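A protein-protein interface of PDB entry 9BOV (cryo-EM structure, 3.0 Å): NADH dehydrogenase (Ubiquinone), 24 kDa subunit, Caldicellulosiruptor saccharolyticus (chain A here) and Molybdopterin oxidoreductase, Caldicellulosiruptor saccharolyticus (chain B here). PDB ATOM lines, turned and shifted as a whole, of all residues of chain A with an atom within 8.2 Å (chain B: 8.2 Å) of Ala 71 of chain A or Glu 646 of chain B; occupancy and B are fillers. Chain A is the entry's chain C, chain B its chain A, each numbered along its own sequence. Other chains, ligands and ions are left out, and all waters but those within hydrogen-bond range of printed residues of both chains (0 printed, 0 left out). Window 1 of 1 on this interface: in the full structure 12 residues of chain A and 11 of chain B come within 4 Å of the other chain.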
ATOM      1  N   LEU A  56      36.454   5.231 -30.157  1.00  0.00           N
ATOM      2  CA  LEU A  56      35.086   5.706 -30.320  1.00  0.00           C
ATOM      3  C   LEU A  56      34.155   4.594 -30.785  1.00  0.00           C
ATOM      4  O   LEU A  56      32.964   4.610 -30.459  1.00  0.00           O
ATOM      5  CB  LEU A  56      35.047   6.880 -31.299  1.00  0.00           C
ATOM      6  CG  LEU A  56      35.390   8.264 -30.742  1.00  0.00           C
ATOM      7  CD1 LEU A  56      34.524   8.584 -29.535  1.00  0.00           C
ATOM      8  CD2 LEU A  56      36.870   8.394 -30.400  1.00  0.00           C
ATOM      9  N   SER A  63      27.643   1.973 -25.710  1.00  0.00           N
ATOM     10  CA  SER A  63      26.418   2.765 -25.693  1.00  0.00           C
ATOM     11  C   SER A  63      25.249   1.983 -26.275  1.00  0.00           C
ATOM     12  O   SER A  63      24.128   2.044 -25.754  1.00  0.00           O
ATOM     13  CB  SER A  63      26.629   4.065 -26.464  1.00  0.00           C
ATOM     14  OG  SER A  63      27.708   4.804 -25.923  1.00  0.00           O
ATOM     15  N   VAL A  68      22.902   3.177 -22.256  1.00  0.00           N
ATOM     16  CA  VAL A  68      23.151   4.495 -21.684  1.00  0.00           C
ATOM     17  C   VAL A  68      23.420   5.467 -22.822  1.00  0.00           C
ATOM     18  O   VAL A  68      23.973   5.098 -23.863  1.00  0.00           O
ATOM     19  CB  VAL A  68      24.323   4.461 -20.681  1.00  0.00           C
ATOM     20  CG1 VAL A  68      24.460   5.796 -19.973  1.00  0.00           C
ATOM     21  CG2 VAL A  68      24.112   3.363 -19.668  1.00  0.00           C
ATOM     22  N   LYS A  69      23.016   6.718 -22.628  1.00  0.00           N
ATOM     23  CA  LYS A  69      23.192   7.722 -23.664  1.00  0.00           C
ATOM     24  C   LYS A  69      24.672   7.974 -23.920  1.00  0.00           C
ATOM     25  O   LYS A  69      25.505   7.918 -23.012  1.00  0.00           O
ATOM     26  CB  LYS A  69      22.488   9.017 -23.269  1.00  0.00           C
ATOM     27  CG  LYS A  69      20.971   8.910 -23.294  1.00  0.00           C
ATOM     28  CD  LYS A  69      20.483   8.133 -24.508  1.00  0.00           C
ATOM     29  CE  LYS A  69      18.982   8.287 -24.686  1.00  0.00           C
ATOM     30  NZ  LYS A  69      18.272   8.367 -23.379  1.00  0.00           N
ATOM     31  N   LYS A  70      24.993   8.249 -25.185  1.00  0.00           N
ATOM     32  CA  LYS A  70      26.387   8.347 -25.608  1.00  0.00           C
ATOM     33  C   LYS A  70      27.100   9.517 -24.940  1.00  0.00           C
ATOM     34  O   LYS A  70      28.284   9.413 -24.590  1.00  0.00           O
ATOM     35  CB  LYS A  70      26.449   8.471 -27.128  1.00  0.00           C
ATOM     36  CG  LYS A  70      25.278   7.811 -27.838  1.00  0.00           C
ATOM     37  CD  LYS A  70      25.708   7.148 -29.134  1.00  0.00           C
ATOM     38  CE  LYS A  70      24.507   6.803 -30.001  1.00  0.00           C
ATOM     39  NZ  LYS A  70      23.682   5.716 -29.404  1.00  0.00           N
ATOM     40  N   ALA A  71      26.403  10.643 -24.774  1.00  0.00           N
ATOM     41  CA  ALA A  71      27.013  11.803 -24.134  1.00  0.00           C
ATOM     42  C   ALA A  71      27.452  11.479 -22.714  1.00  0.00           C
ATOM     43  O   ALA A  71      28.518  11.919 -22.271  1.00  0.00           O
ATOM     44  CB  ALA A  71      26.038  12.980 -24.138  1.00  0.00           C
ATOM     45  N   LYS A  72      26.640  10.712 -21.984  1.00  0.00           N
ATOM     46  CA  LYS A  72      27.029  10.280 -20.648  1.00  0.00           C
ATOM     47  C   LYS A  72      28.300   9.444 -20.694  1.00  0.00           C
ATOM     48  O   LYS A  72      29.185   9.593 -19.842  1.00  0.00           O
ATOM     49  CB  LYS A  72      25.889   9.491 -20.008  1.00  0.00           C
ATOM     50  CG  LYS A  72      26.096   9.160 -18.547  1.00  0.00           C
ATOM     51  CD  LYS A  72      24.761   8.945 -17.852  1.00  0.00           C
ATOM     52  CE  LYS A  72      24.151  10.263 -17.405  1.00  0.00           C
ATOM     53  NZ  LYS A  72      23.358  10.110 -16.155  1.00  0.00           N
ATOM     54  N   ILE A  73      28.405   8.560 -21.688  1.00  0.00           N
ATOM     55  CA  ILE A  73      29.590   7.717 -21.821  1.00  0.00           C
ATOM     56  C   ILE A  73      30.825   8.577 -22.035  1.00  0.00           C
ATOM     57  O   ILE A  73      31.858   8.388 -21.385  1.00  0.00           O
ATOM     58  CB  ILE A  73      29.413   6.712 -22.973  1.00  0.00           C
ATOM     59  CG1 ILE A  73      28.099   5.940 -22.844  1.00  0.00           C
ATOM     60  CG2 ILE A  73      30.581   5.753 -23.012  1.00  0.00           C
ATOM     61  CD1 ILE A  73      27.783   5.467 -21.453  1.00  0.00           C
ATOM     62  N   TYR A  74      30.733   9.545 -22.949  1.00  0.00           N
ATOM     63  CA  TYR A  74      31.895  10.383 -23.228  1.00  0.00           C
ATOM     64  C   TYR A  74      32.250  11.259 -22.034  1.00  0.00           C
ATOM     65  O   TYR A  74      33.433  11.494 -21.763  1.00  0.00           O
ATOM     66  CB  TYR A  74      31.651  11.234 -24.471  1.00  0.00           C
ATOM     67  CG  TYR A  74      32.920  11.606 -25.201  1.00  0.00           C
ATOM     68  CD1 TYR A  74      33.444  10.781 -26.185  1.00  0.00           C
ATOM     69  CD2 TYR A  74      33.605  12.769 -24.892  1.00  0.00           C
ATOM     70  CE1 TYR A  74      34.606  11.114 -26.855  1.00  0.00           C
ATOM     71  CE2 TYR A  74      34.765  13.113 -25.556  1.00  0.00           C
ATOM     72  CZ  TYR A  74      35.264  12.281 -26.535  1.00  0.00           C
ATOM     73  OH  TYR A  74      36.423  12.619 -27.196  1.00  0.00           O
ATOM     74  N   GLY A  75      31.243  11.750 -21.308  1.00  0.00           N
ATOM     75  CA  GLY A  75      31.525  12.558 -20.132  1.00  0.00           C
ATOM     76  C   GLY A  75      32.233  11.773 -19.046  1.00  0.00           C
ATOM     77  O   GLY A  75      33.236  12.224 -18.485  1.00  0.00           O
ATOM     78  N   ILE A  76      31.731  10.573 -18.745  1.00  0.00           N
ATOM     79  CA  ILE A  76      32.377   9.754 -17.727  1.00  0.00           C
ATOM     80  C   ILE A  76      33.745   9.275 -18.202  1.00  0.00           C
ATOM     81  O   ILE A  76      34.636   9.018 -17.386  1.00  0.00           O
ATOM     82  CB  ILE A  76      31.460   8.585 -17.316  1.00  0.00           C
ATOM     83  CG1 ILE A  76      31.984   7.910 -16.053  1.00  0.00           C
ATOM     84  CG2 ILE A  76      31.332   7.572 -18.423  1.00  0.00           C
ATOM     85  CD1 ILE A  76      31.957   8.794 -14.840  1.00  0.00           C
ATOM     86  N   ALA A  77      33.945   9.154 -19.518  1.00  0.00           N
ATOM     87  CA  ALA A  77      35.244   8.730 -20.025  1.00  0.00           C
ATOM     88  C   ALA A  77      36.274   9.846 -19.923  1.00  0.00           C
ATOM     89  O   ALA A  77      37.419   9.605 -19.529  1.00  0.00           O
ATOM     90  CB  ALA A  77      35.115   8.257 -21.470  1.00  0.00           C
ATOM     91  N   THR A  78      35.890  11.071 -20.271  1.00  0.00           N
ATOM     92  CA  THR A  78      36.836  12.178 -20.249  1.00  0.00           C
ATOM     93  C   THR A  78      36.966  12.828 -18.879  1.00  0.00           C
ATOM     94  O   THR A  78      37.865  13.654 -18.693  1.00  0.00           O
ATOM     95  CB  THR A  78      36.436  13.240 -21.273  1.00  0.00           C
ATOM     96  OG1 THR A  78      35.049  13.564 -21.114  1.00  0.00           O
ATOM     97  CG2 THR A  78      36.676  12.733 -22.677  1.00  0.00           C
ATOM     98  N   ILE B 620      22.634  21.157 -21.587  1.00  0.00           N
ATOM     99  CA  ILE B 620      22.654  19.739 -21.237  1.00  0.00           C
ATOM    100  C   ILE B 620      21.429  19.381 -20.409  1.00  0.00           C
ATOM    101  O   ILE B 620      20.757  18.372 -20.657  1.00  0.00           O
ATOM    102  CB  ILE B 620      23.954  19.394 -20.491  1.00  0.00           C
ATOM    103  CG1 ILE B 620      25.165  19.696 -21.367  1.00  0.00           C
ATOM    104  CG2 ILE B 620      23.951  17.944 -20.059  1.00  0.00           C
ATOM    105  CD1 ILE B 620      26.407  19.983 -20.585  1.00  0.00           C
ATOM    106  N   CYS B 623      18.308  19.392 -22.611  1.00  0.00           N
ATOM    107  CA  CYS B 623      18.265  18.279 -23.549  1.00  0.00           C
ATOM    108  C   CYS B 623      18.049  16.951 -22.842  1.00  0.00           C
ATOM    109  O   CYS B 623      17.552  16.007 -23.462  1.00  0.00           O
ATOM    110  CB  CYS B 623      19.553  18.230 -24.371  1.00  0.00           C
ATOM    111  SG  CYS B 623      19.501  17.118 -25.794  1.00  0.00           S
ATOM    112  N   GLU B 624      18.408  16.858 -21.563  1.00  0.00           N
ATOM    113  CA  GLU B 624      18.277  15.615 -20.814  1.00  0.00           C
ATOM    114  C   GLU B 624      17.009  15.545 -19.975  1.00  0.00           C
ATOM    115  O   GLU B 624      16.402  14.476 -19.874  1.00  0.00           O
ATOM    116  CB  GLU B 624      19.505  15.427 -19.916  1.00  0.00           C
ATOM    117  CG  GLU B 624      19.223  14.846 -18.545  1.00  0.00           C
ATOM    118  CD  GLU B 624      20.440  14.881 -17.646  1.00  0.00           C
ATOM    119  OE1 GLU B 624      20.312  14.525 -16.455  1.00  0.00           O
ATOM    120  OE2 GLU B 624      21.524  15.268 -18.128  1.00  0.00           O
ATOM    121  N   VAL B 629      16.277  13.643 -25.114  1.00  0.00           N
ATOM    122  CA  VAL B 629      17.160  13.057 -26.116  1.00  0.00           C
ATOM    123  C   VAL B 629      18.550  12.802 -25.546  1.00  0.00           C
ATOM    124  O   VAL B 629      19.176  11.787 -25.860  1.00  0.00           O
ATOM    125  CB  VAL B 629      17.210  13.967 -27.359  1.00  0.00           C
ATOM    126  CG1 VAL B 629      18.382  13.605 -28.246  1.00  0.00           C
ATOM    127  CG2 VAL B 629      15.915  13.867 -28.133  1.00  0.00           C
ATOM    128  N   CYS B 630      19.034  13.708 -24.696  1.00  0.00           N
ATOM    129  CA  CYS B 630      20.353  13.600 -24.070  1.00  0.00           C
ATOM    130  C   CYS B 630      21.460  13.538 -25.121  1.00  0.00           C
ATOM    131  O   CYS B 630      22.306  12.643 -25.114  1.00  0.00           O
ATOM    132  CB  CYS B 630      20.426  12.392 -23.132  1.00  0.00           C
ATOM    133  SG  CYS B 630      19.203  12.352 -21.807  1.00  0.00           S
ATOM    134  N   ALA B 631      21.445  14.504 -26.037  1.00  0.00           N
ATOM    135  CA  ALA B 631      22.431  14.551 -27.109  1.00  0.00           C
ATOM    136  C   ALA B 631      23.654  15.387 -26.768  1.00  0.00           C
ATOM    137  O   ALA B 631      24.626  15.364 -27.528  1.00  0.00           O
ATOM    138  CB  ALA B 631      21.795  15.091 -28.392  1.00  0.00           C
ATOM    139  N   LEU B 632      23.636  16.118 -25.658  1.00  0.00           N
ATOM    140  CA  LEU B 632      24.758  16.934 -25.224  1.00  0.00           C
ATOM    141  C   LEU B 632      25.286  16.410 -23.898  1.00  0.00           C
ATOM    142  O   LEU B 632      24.572  15.752 -23.139  1.00  0.00           O
ATOM    143  CB  LEU B 632      24.361  18.406 -25.067  1.00  0.00           C
ATOM    144  CG  LEU B 632      23.768  19.126 -26.273  1.00  0.00           C
ATOM    145  CD1 LEU B 632      23.214  20.466 -25.849  1.00  0.00           C
ATOM    146  CD2 LEU B 632      24.807  19.299 -27.354  1.00  0.00           C
ATOM    147  N   GLY B 633      26.546  16.716 -23.618  1.00  0.00           N
ATOM    148  CA  GLY B 633      27.124  16.331 -22.348  1.00  0.00           C
ATOM    149  C   GLY B 633      28.422  17.057 -22.093  1.00  0.00           C
ATOM    150  O   GLY B 633      29.048  17.600 -23.009  1.00  0.00           O
ATOM    151  N   PHE B 634      28.819  17.055 -20.826  1.00  0.00           N
ATOM    152  CA  PHE B 634      30.105  17.615 -20.448  1.00  0.00           C
ATOM    153  C   PHE B 634      31.234  16.715 -20.932  1.00  0.00           C
ATOM    154  O   PHE B 634      31.078  15.500 -21.065  1.00  0.00           O
ATOM    155  CB  PHE B 634      30.186  17.789 -18.933  1.00  0.00           C
ATOM    156  CG  PHE B 634      29.400  18.954 -18.417  1.00  0.00           C
ATOM    157  CD1 PHE B 634      29.722  20.244 -18.792  1.00  0.00           C
ATOM    158  CD2 PHE B 634      28.337  18.758 -17.556  1.00  0.00           C
ATOM    159  CE1 PHE B 634      28.999  21.317 -18.318  1.00  0.00           C
ATOM    160  CE2 PHE B 634      27.611  19.828 -17.080  1.00  0.00           C
ATOM    161  CZ  PHE B 634      27.944  21.109 -17.461  1.00  0.00           C
ATOM    162  N   VAL B 635      32.378  17.329 -21.211  1.00  0.00           N
ATOM    163  CA  VAL B 635      33.566  16.629 -21.676  1.00  0.00           C
ATOM    164  C   VAL B 635      34.761  17.235 -20.955  1.00  0.00           C
ATOM    165  O   VAL B 635      34.784  18.443 -20.686  1.00  0.00           O
ATOM    166  CB  VAL B 635      33.720  16.729 -23.210  1.00  0.00           C
ATOM    167  CG1 VAL B 635      35.055  16.172 -23.667  1.00  0.00           C
ATOM    168  CG2 VAL B 635      32.588  16.002 -23.909  1.00  0.00           C
ATOM    169  N   VAL B 643      31.194  21.677 -23.346  1.00  0.00           N
ATOM    170  CA  VAL B 643      29.933  21.029 -23.689  1.00  0.00           C
ATOM    171  C   VAL B 643      30.031  20.517 -25.119  1.00  0.00           C
ATOM    172  O   VAL B 643      30.269  21.293 -26.051  1.00  0.00           O
ATOM    173  CB  VAL B 643      28.751  21.992 -23.524  1.00  0.00           C
ATOM    174  CG1 VAL B 643      27.468  21.321 -23.965  1.00  0.00           C
ATOM    175  CG2 VAL B 643      28.654  22.459 -22.085  1.00  0.00           C
ATOM    176  N   LYS B 644      29.853  19.214 -25.299  1.00  0.00           N
ATOM    177  CA  LYS B 644      29.987  18.614 -26.614  1.00  0.00           C
ATOM    178  C   LYS B 644      28.843  17.649 -26.877  1.00  0.00           C
ATOM    179  O   LYS B 644      28.263  17.090 -25.941  1.00  0.00           O
ATOM    180  CB  LYS B 644      31.321  17.870 -26.752  1.00  0.00           C
ATOM    181  CG  LYS B 644      32.427  18.689 -27.384  1.00  0.00           C
ATOM    182  CD  LYS B 644      33.792  18.120 -27.044  1.00  0.00           C
ATOM    183  CE  LYS B 644      34.665  18.011 -28.280  1.00  0.00           C
ATOM    184  NZ  LYS B 644      36.104  17.880 -27.931  1.00  0.00           N
ATOM    185  N   PRO B 645      28.502  17.432 -28.145  1.00  0.00           N
ATOM    186  CA  PRO B 645      27.489  16.422 -28.476  1.00  0.00           C
ATOM    187  C   PRO B 645      27.982  15.007 -28.215  1.00  0.00           C
ATOM    188  O   PRO B 645      29.080  14.815 -27.687  1.00  0.00           O
ATOM    189  CB  PRO B 645      27.228  16.659 -29.968  1.00  0.00           C
ATOM    190  CG  PRO B 645      27.736  18.032 -30.241  1.00  0.00           C
ATOM    191  CD  PRO B 645      28.887  18.229 -29.319  1.00  0.00           C
ATOM    192  N   GLU B 646      27.169  14.015 -28.569  1.00  0.00           N
ATOM    193  CA  GLU B 646      27.534  12.620 -28.347  1.00  0.00           C
ATOM    194  C   GLU B 646      28.849  12.290 -29.039  1.00  0.00           C
ATOM    195  O   GLU B 646      28.950  12.362 -30.268  1.00  0.00           O
ATOM    196  CB  GLU B 646      26.422  11.705 -28.856  1.00  0.00           C
ATOM    197  CG  GLU B 646      25.143  11.776 -28.047  1.00  0.00           C
ATOM    198  CD  GLU B 646      24.008  11.002 -28.682  1.00  0.00           C
ATOM    199  OE1 GLU B 646      23.985  10.891 -29.925  1.00  0.00           O
ATOM    200  OE2 GLU B 646      23.137  10.505 -27.940  1.00  0.00           O
ATOM    201  N   PHE B 647      29.856  11.930 -28.240  1.00  0.00           N
ATOM    202  CA  PHE B 647      31.186  11.557 -28.728  1.00  0.00           C
ATOM    203  C   PHE B 647      31.851  12.687 -29.507  1.00  0.00           C
ATOM    204  O   PHE B 647      32.697  12.444 -30.370  1.00  0.00           O
ATOM    205  CB  PHE B 647      31.136  10.288 -29.584  1.00  0.00           C
ATOM    206  CG  PHE B 647      30.648   9.078 -28.845  1.00  0.00           C
ATOM    207  CD1 PHE B 647      31.178   8.741 -27.615  1.00  0.00           C
ATOM    208  CD2 PHE B 647      29.668   8.268 -29.387  1.00  0.00           C
ATOM    209  CE1 PHE B 647      30.731   7.632 -26.933  1.00  0.00           C
ATOM    210  CE2 PHE B 647      29.221   7.154 -28.712  1.00  0.00           C
ATOM    211  CZ  PHE B 647      29.753   6.836 -27.481  1.00  0.00           C
ATOM    212  N   GLY B 648      31.481  13.932 -29.212  1.00  0.00           N
ATOM    213  CA  GLY B 648      32.060  15.070 -29.899  1.00  0.00           C
ATOM    214  C   GLY B 648      31.704  15.121 -31.369  1.00  0.00           C
ATOM    215  O   GLY B 648      32.311  15.870 -32.140  1.00  0.00           O
ATOM    216  N   LEU B 649      30.719  14.321 -31.767  1.00  0.00           N
ATOM    217  CA  LEU B 649      30.285  14.270 -33.148  1.00  0.00           C
ATOM    218  C   LEU B 649      29.536  15.547 -33.517  1.00  0.00           C
ATOM    219  O   LEU B 649      29.082  16.285 -32.642  1.00  0.00           O
ATOM    220  CB  LEU B 649      29.390  13.054 -33.374  1.00  0.00           C
ATOM    221  CG  LEU B 649      30.064  11.684 -33.372  1.00  0.00           C
ATOM    222  CD1 LEU B 649      29.023  10.581 -33.310  1.00  0.00           C
ATOM    223  CD2 LEU B 649      30.940  11.523 -34.597  1.00  0.00           C
ATOM    224  N   PRO B 650      29.409  15.837 -34.811  1.00  0.00           N
ATOM    225  CA  PRO B 650      28.541  16.942 -35.224  1.00  0.00           C
ATOM    226  C   PRO B 650      27.106  16.689 -34.790  1.00  0.00           C
ATOM    227  O   PRO B 650      26.668  15.545 -34.658  1.00  0.00           O
ATOM    228  CB  PRO B 650      28.675  16.949 -36.751  1.00  0.00           C
ATOM    229  CG  PRO B 650      29.981  16.302 -37.014  1.00  0.00           C
ATOM    230  CD  PRO B 650      30.156  15.270 -35.945  1.00  0.00           C
ATOM    231  N   LEU B 651      26.378  17.783 -34.552  1.00  0.00           N
ATOM    232  CA  LEU B 651      25.020  17.675 -34.027  1.00  0.00           C
ATOM    233  C   LEU B 651      24.124  16.838 -34.930  1.00  0.00           C
ATOM    234  O   LEU B 651      23.179  16.206 -34.448  1.00  0.00           O
ATOM    235  CB  LEU B 651      24.424  19.070 -33.832  1.00  0.00           C
ATOM    236  CG  LEU B 651      23.620  19.332 -32.559  1.00  0.00           C
ATOM    237  CD1 LEU B 651      24.332  18.773 -31.345  1.00  0.00           C
ATOM    238  CD2 LEU B 651      23.370  20.816 -32.392  1.00  0.00           C
ATOM    239  N   GLU B 652      24.401  16.816 -36.235  1.00  0.00           N
ATOM    240  CA  GLU B 652      23.572  16.035 -37.147  1.00  0.00           C
ATOM    241  C   GLU B 652      23.846  14.542 -37.031  1.00  0.00           C
ATOM    242  O   GLU B 652      22.950  13.731 -37.286  1.00  0.00           O
ATOM    243  CB  GLU B 652      23.789  16.503 -38.586  1.00  0.00           C
ATOM    244  CG  GLU B 652      25.228  16.439 -39.046  1.00  0.00           C
ATOM    245  CD  GLU B 652      25.908  17.788 -39.003  1.00  0.00           C
ATOM    246  OE1 GLU B 652      25.628  18.563 -38.066  1.00  0.00           O
ATOM    247  OE2 GLU B 652      26.721  18.074 -39.904  1.00  0.00           O
ATOM    248  N   GLU B 653      25.065  14.157 -36.655  1.00  0.00           N
ATOM    249  CA  GLU B 653      25.405  12.746 -36.536  1.00  0.00           C
ATOM    250  C   GLU B 653      24.995  12.145 -35.200  1.00  0.00           C
ATOM    251  O   GLU B 653      25.131  10.931 -35.018  1.00  0.00           O
ATOM    252  CB  GLU B 653      26.906  12.547 -36.746  1.00  0.00           C
ATOM    253  CG  GLU B 653      27.492  13.419 -37.838  1.00  0.00           C
ATOM    254  CD  GLU B 653      28.645  12.752 -38.557  1.00  0.00           C
ATOM    255  OE1 GLU B 653      29.232  11.805 -37.993  1.00  0.00           O
ATOM    256  OE2 GLU B 653      28.964  13.174 -39.688  1.00  0.00           O
ATOM    257  N   THR B 654      24.507  12.955 -34.270  1.00  0.00           N
ATOM    258  CA  THR B 654      24.042  12.469 -32.982  1.00  0.00           C
ATOM    259  C   THR B 654      22.545  12.183 -33.062  1.00  0.00           C
ATOM    260  O   THR B 654      21.949  12.168 -34.141  1.00  0.00           O
ATOM    261  CB  THR B 654      24.374  13.476 -31.886  1.00  0.00           C
ATOM    262  OG1 THR B 654      23.643  14.686 -32.113  1.00  0.00           O
ATOM    263  CG2 THR B 654      25.857  13.785 -31.886  1.00  0.00           C
ATOM    264  N   SER B 655      21.921  11.950 -31.913  1.00  0.00           N
ATOM    265  CA  SER B 655      20.484  11.732 -31.838  1.00  0.00           C
ATOM    266  C   SER B 655      19.706  13.030 -31.689  1.00  0.00           C
ATOM    267  O   SER B 655      18.496  12.988 -31.446  1.00  0.00           O
ATOM    268  CB  SER B 655      20.153  10.791 -30.680  1.00  0.00           C
ATOM    269  OG  SER B 655      20.722  11.256 -29.470  1.00  0.00           O
ATOM    270  N   CYS B 656      20.373  14.174 -31.819  1.00  0.00           N
ATOM    271  CA  CYS B 656      19.706  15.462 -31.694  1.00  0.00           C
ATOM    272  C   CYS B 656      18.579  15.581 -32.711  1.00  0.00           C
ATOM    273  O   CYS B 656      18.733  15.226 -33.881  1.00  0.00           O
ATOM    274  CB  CYS B 656      20.716  16.594 -31.884  1.00  0.00           C
ATOM    275  SG  CYS B 656      20.009  18.154 -32.435  1.00  0.00           S
ATOM    276  N   LYS B1177      17.152  14.884 -38.081  1.00  0.00           N
ATOM    277  CA  LYS B1177      15.974  14.248 -37.511  1.00  0.00           C
ATOM    278  C   LYS B1177      15.027  15.316 -36.973  1.00  0.00           C
ATOM    279  O   LYS B1177      15.318  16.515 -37.000  1.00  0.00           O
ATOM    280  CB  LYS B1177      16.369  13.262 -36.411  1.00  0.00           C
ATOM    281  CG  LYS B1177      17.454  12.278 -36.805  1.00  0.00           C
ATOM    282  CD  LYS B1177      17.739  11.301 -35.676  1.00  0.00           C
ATOM    283  CE  LYS B1177      19.147  10.733 -35.769  1.00  0.00           C
ATOM    284  NZ  LYS B1177      19.983  11.461 -36.762  1.00  0.00           N
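Printed residues of chain B that touch a printed residue of chain A: Val 629, Cys 630, Leu 632, Gly 633, Phe 634, Val 635, Glu 646 and Phe 647.
Hydrophobic or aromatic side chains of chain B within 4 Å of the printed part of chain A: Val 635 and Phe 647.
Hydrophobic or aromatic side chains of chain A that line the printed part of chain B: Leu 56, Ala 71 and Tyr 74.
Among the printed residues, no Asp or Glu carboxylate lies within 4 Å of a Lys or Arg side-chain nitrogen of the other chain.
N of Val 629 of chain B is in hydrogen-bond range of O of Cys 623 of chain B.
O of Ala 631 of chain B is in hydrogen-bond range of N of Glu 646 of chain B (3.1 Å).
N of Gly 633 of chain B sits at hydrogen-bond distance from O of Lys 644 of chain B.
The side-chain hydroxyl (OG) of Ser 655 of chain B is in hydrogen-bond range of the side-chain carboxylate (OE2) of Glu 646 of chain B (3.0 Å).
OG1 of Thr 78 of chain A sits at hydrogen-bond distance from O of Tyr 74 of chain A (2.7 Å).
OG1 of Thr 78 of chain A is in hydrogen-bond range of O of Gly 75 of chain A (3.5 Å).
Among the printed residues, merely in contact across the chains: Leu 56 of chain A with Phe 647 of chain B (3.8 Å), Ser 63 of chain A with Phe 647 of chain B (3.3 Å), Lys 69 of chain A with Val 629 of chain B (3.7 Å), Lys 69 of chain A with Cys 630 of chain B (3.5 Å), Lys 70 of chain A with Glu 646 of chain B (3.4 Å), Lys 70 of chain A with Phe 647 of chain B (3.5 Å), Ala 71 of chain A with Cys 630 of chain B (3.9 Å), Ala 71 of chain A with Leu 632 of chain B (3.3 Å), Ala 71 of chain A with Gly 633 of chain B (3.8 Å), Ala 71 of chain A with Glu 646 of chain B (3.7 Å), Tyr 74 of chain A with Val 635 of chain B (3.5 Å), Tyr 74 of chain A with Phe 647 of chain B (3.4 Å), Gly 75 of chain A with Phe 634 of chain B (3.1 Å) and Thr 78 of chain A with Val 635 of chain B (3.5 Å).
Of the printed residues of chain B, Ala 71 of chain A touches Cys 630 (3.9 Å), Leu 632 (3.3 Å), Gly 633 (3.8 Å) and Glu 646 (3.7 Å).
Of the printed residues of chain A, Phe 647 of chain B touches Leu 56 (3.8 Å), Ser 63 (3.3 Å), Lys 70 (3.5 Å) and Tyr 74 (3.4 Å).
Printed residues of chain A within 4 Å of Phe 634 of chain B: Gly 75 (3.1 Å).
Of the printed residues of chain A, Val 635 of chain B touches Tyr 74 (3.5 Å) and Thr 78 (3.5 Å).
Printed residues of chain B within 4 Å of Thr 78 of chain A: Val 635 (3.5 Å).
Glu 624 of chain B touches none of the printed residues of chain A.
The nearest printed residue of chain A that does not touch Leu 632 of chain B is Lys 72 of chain A (5.6 Å).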
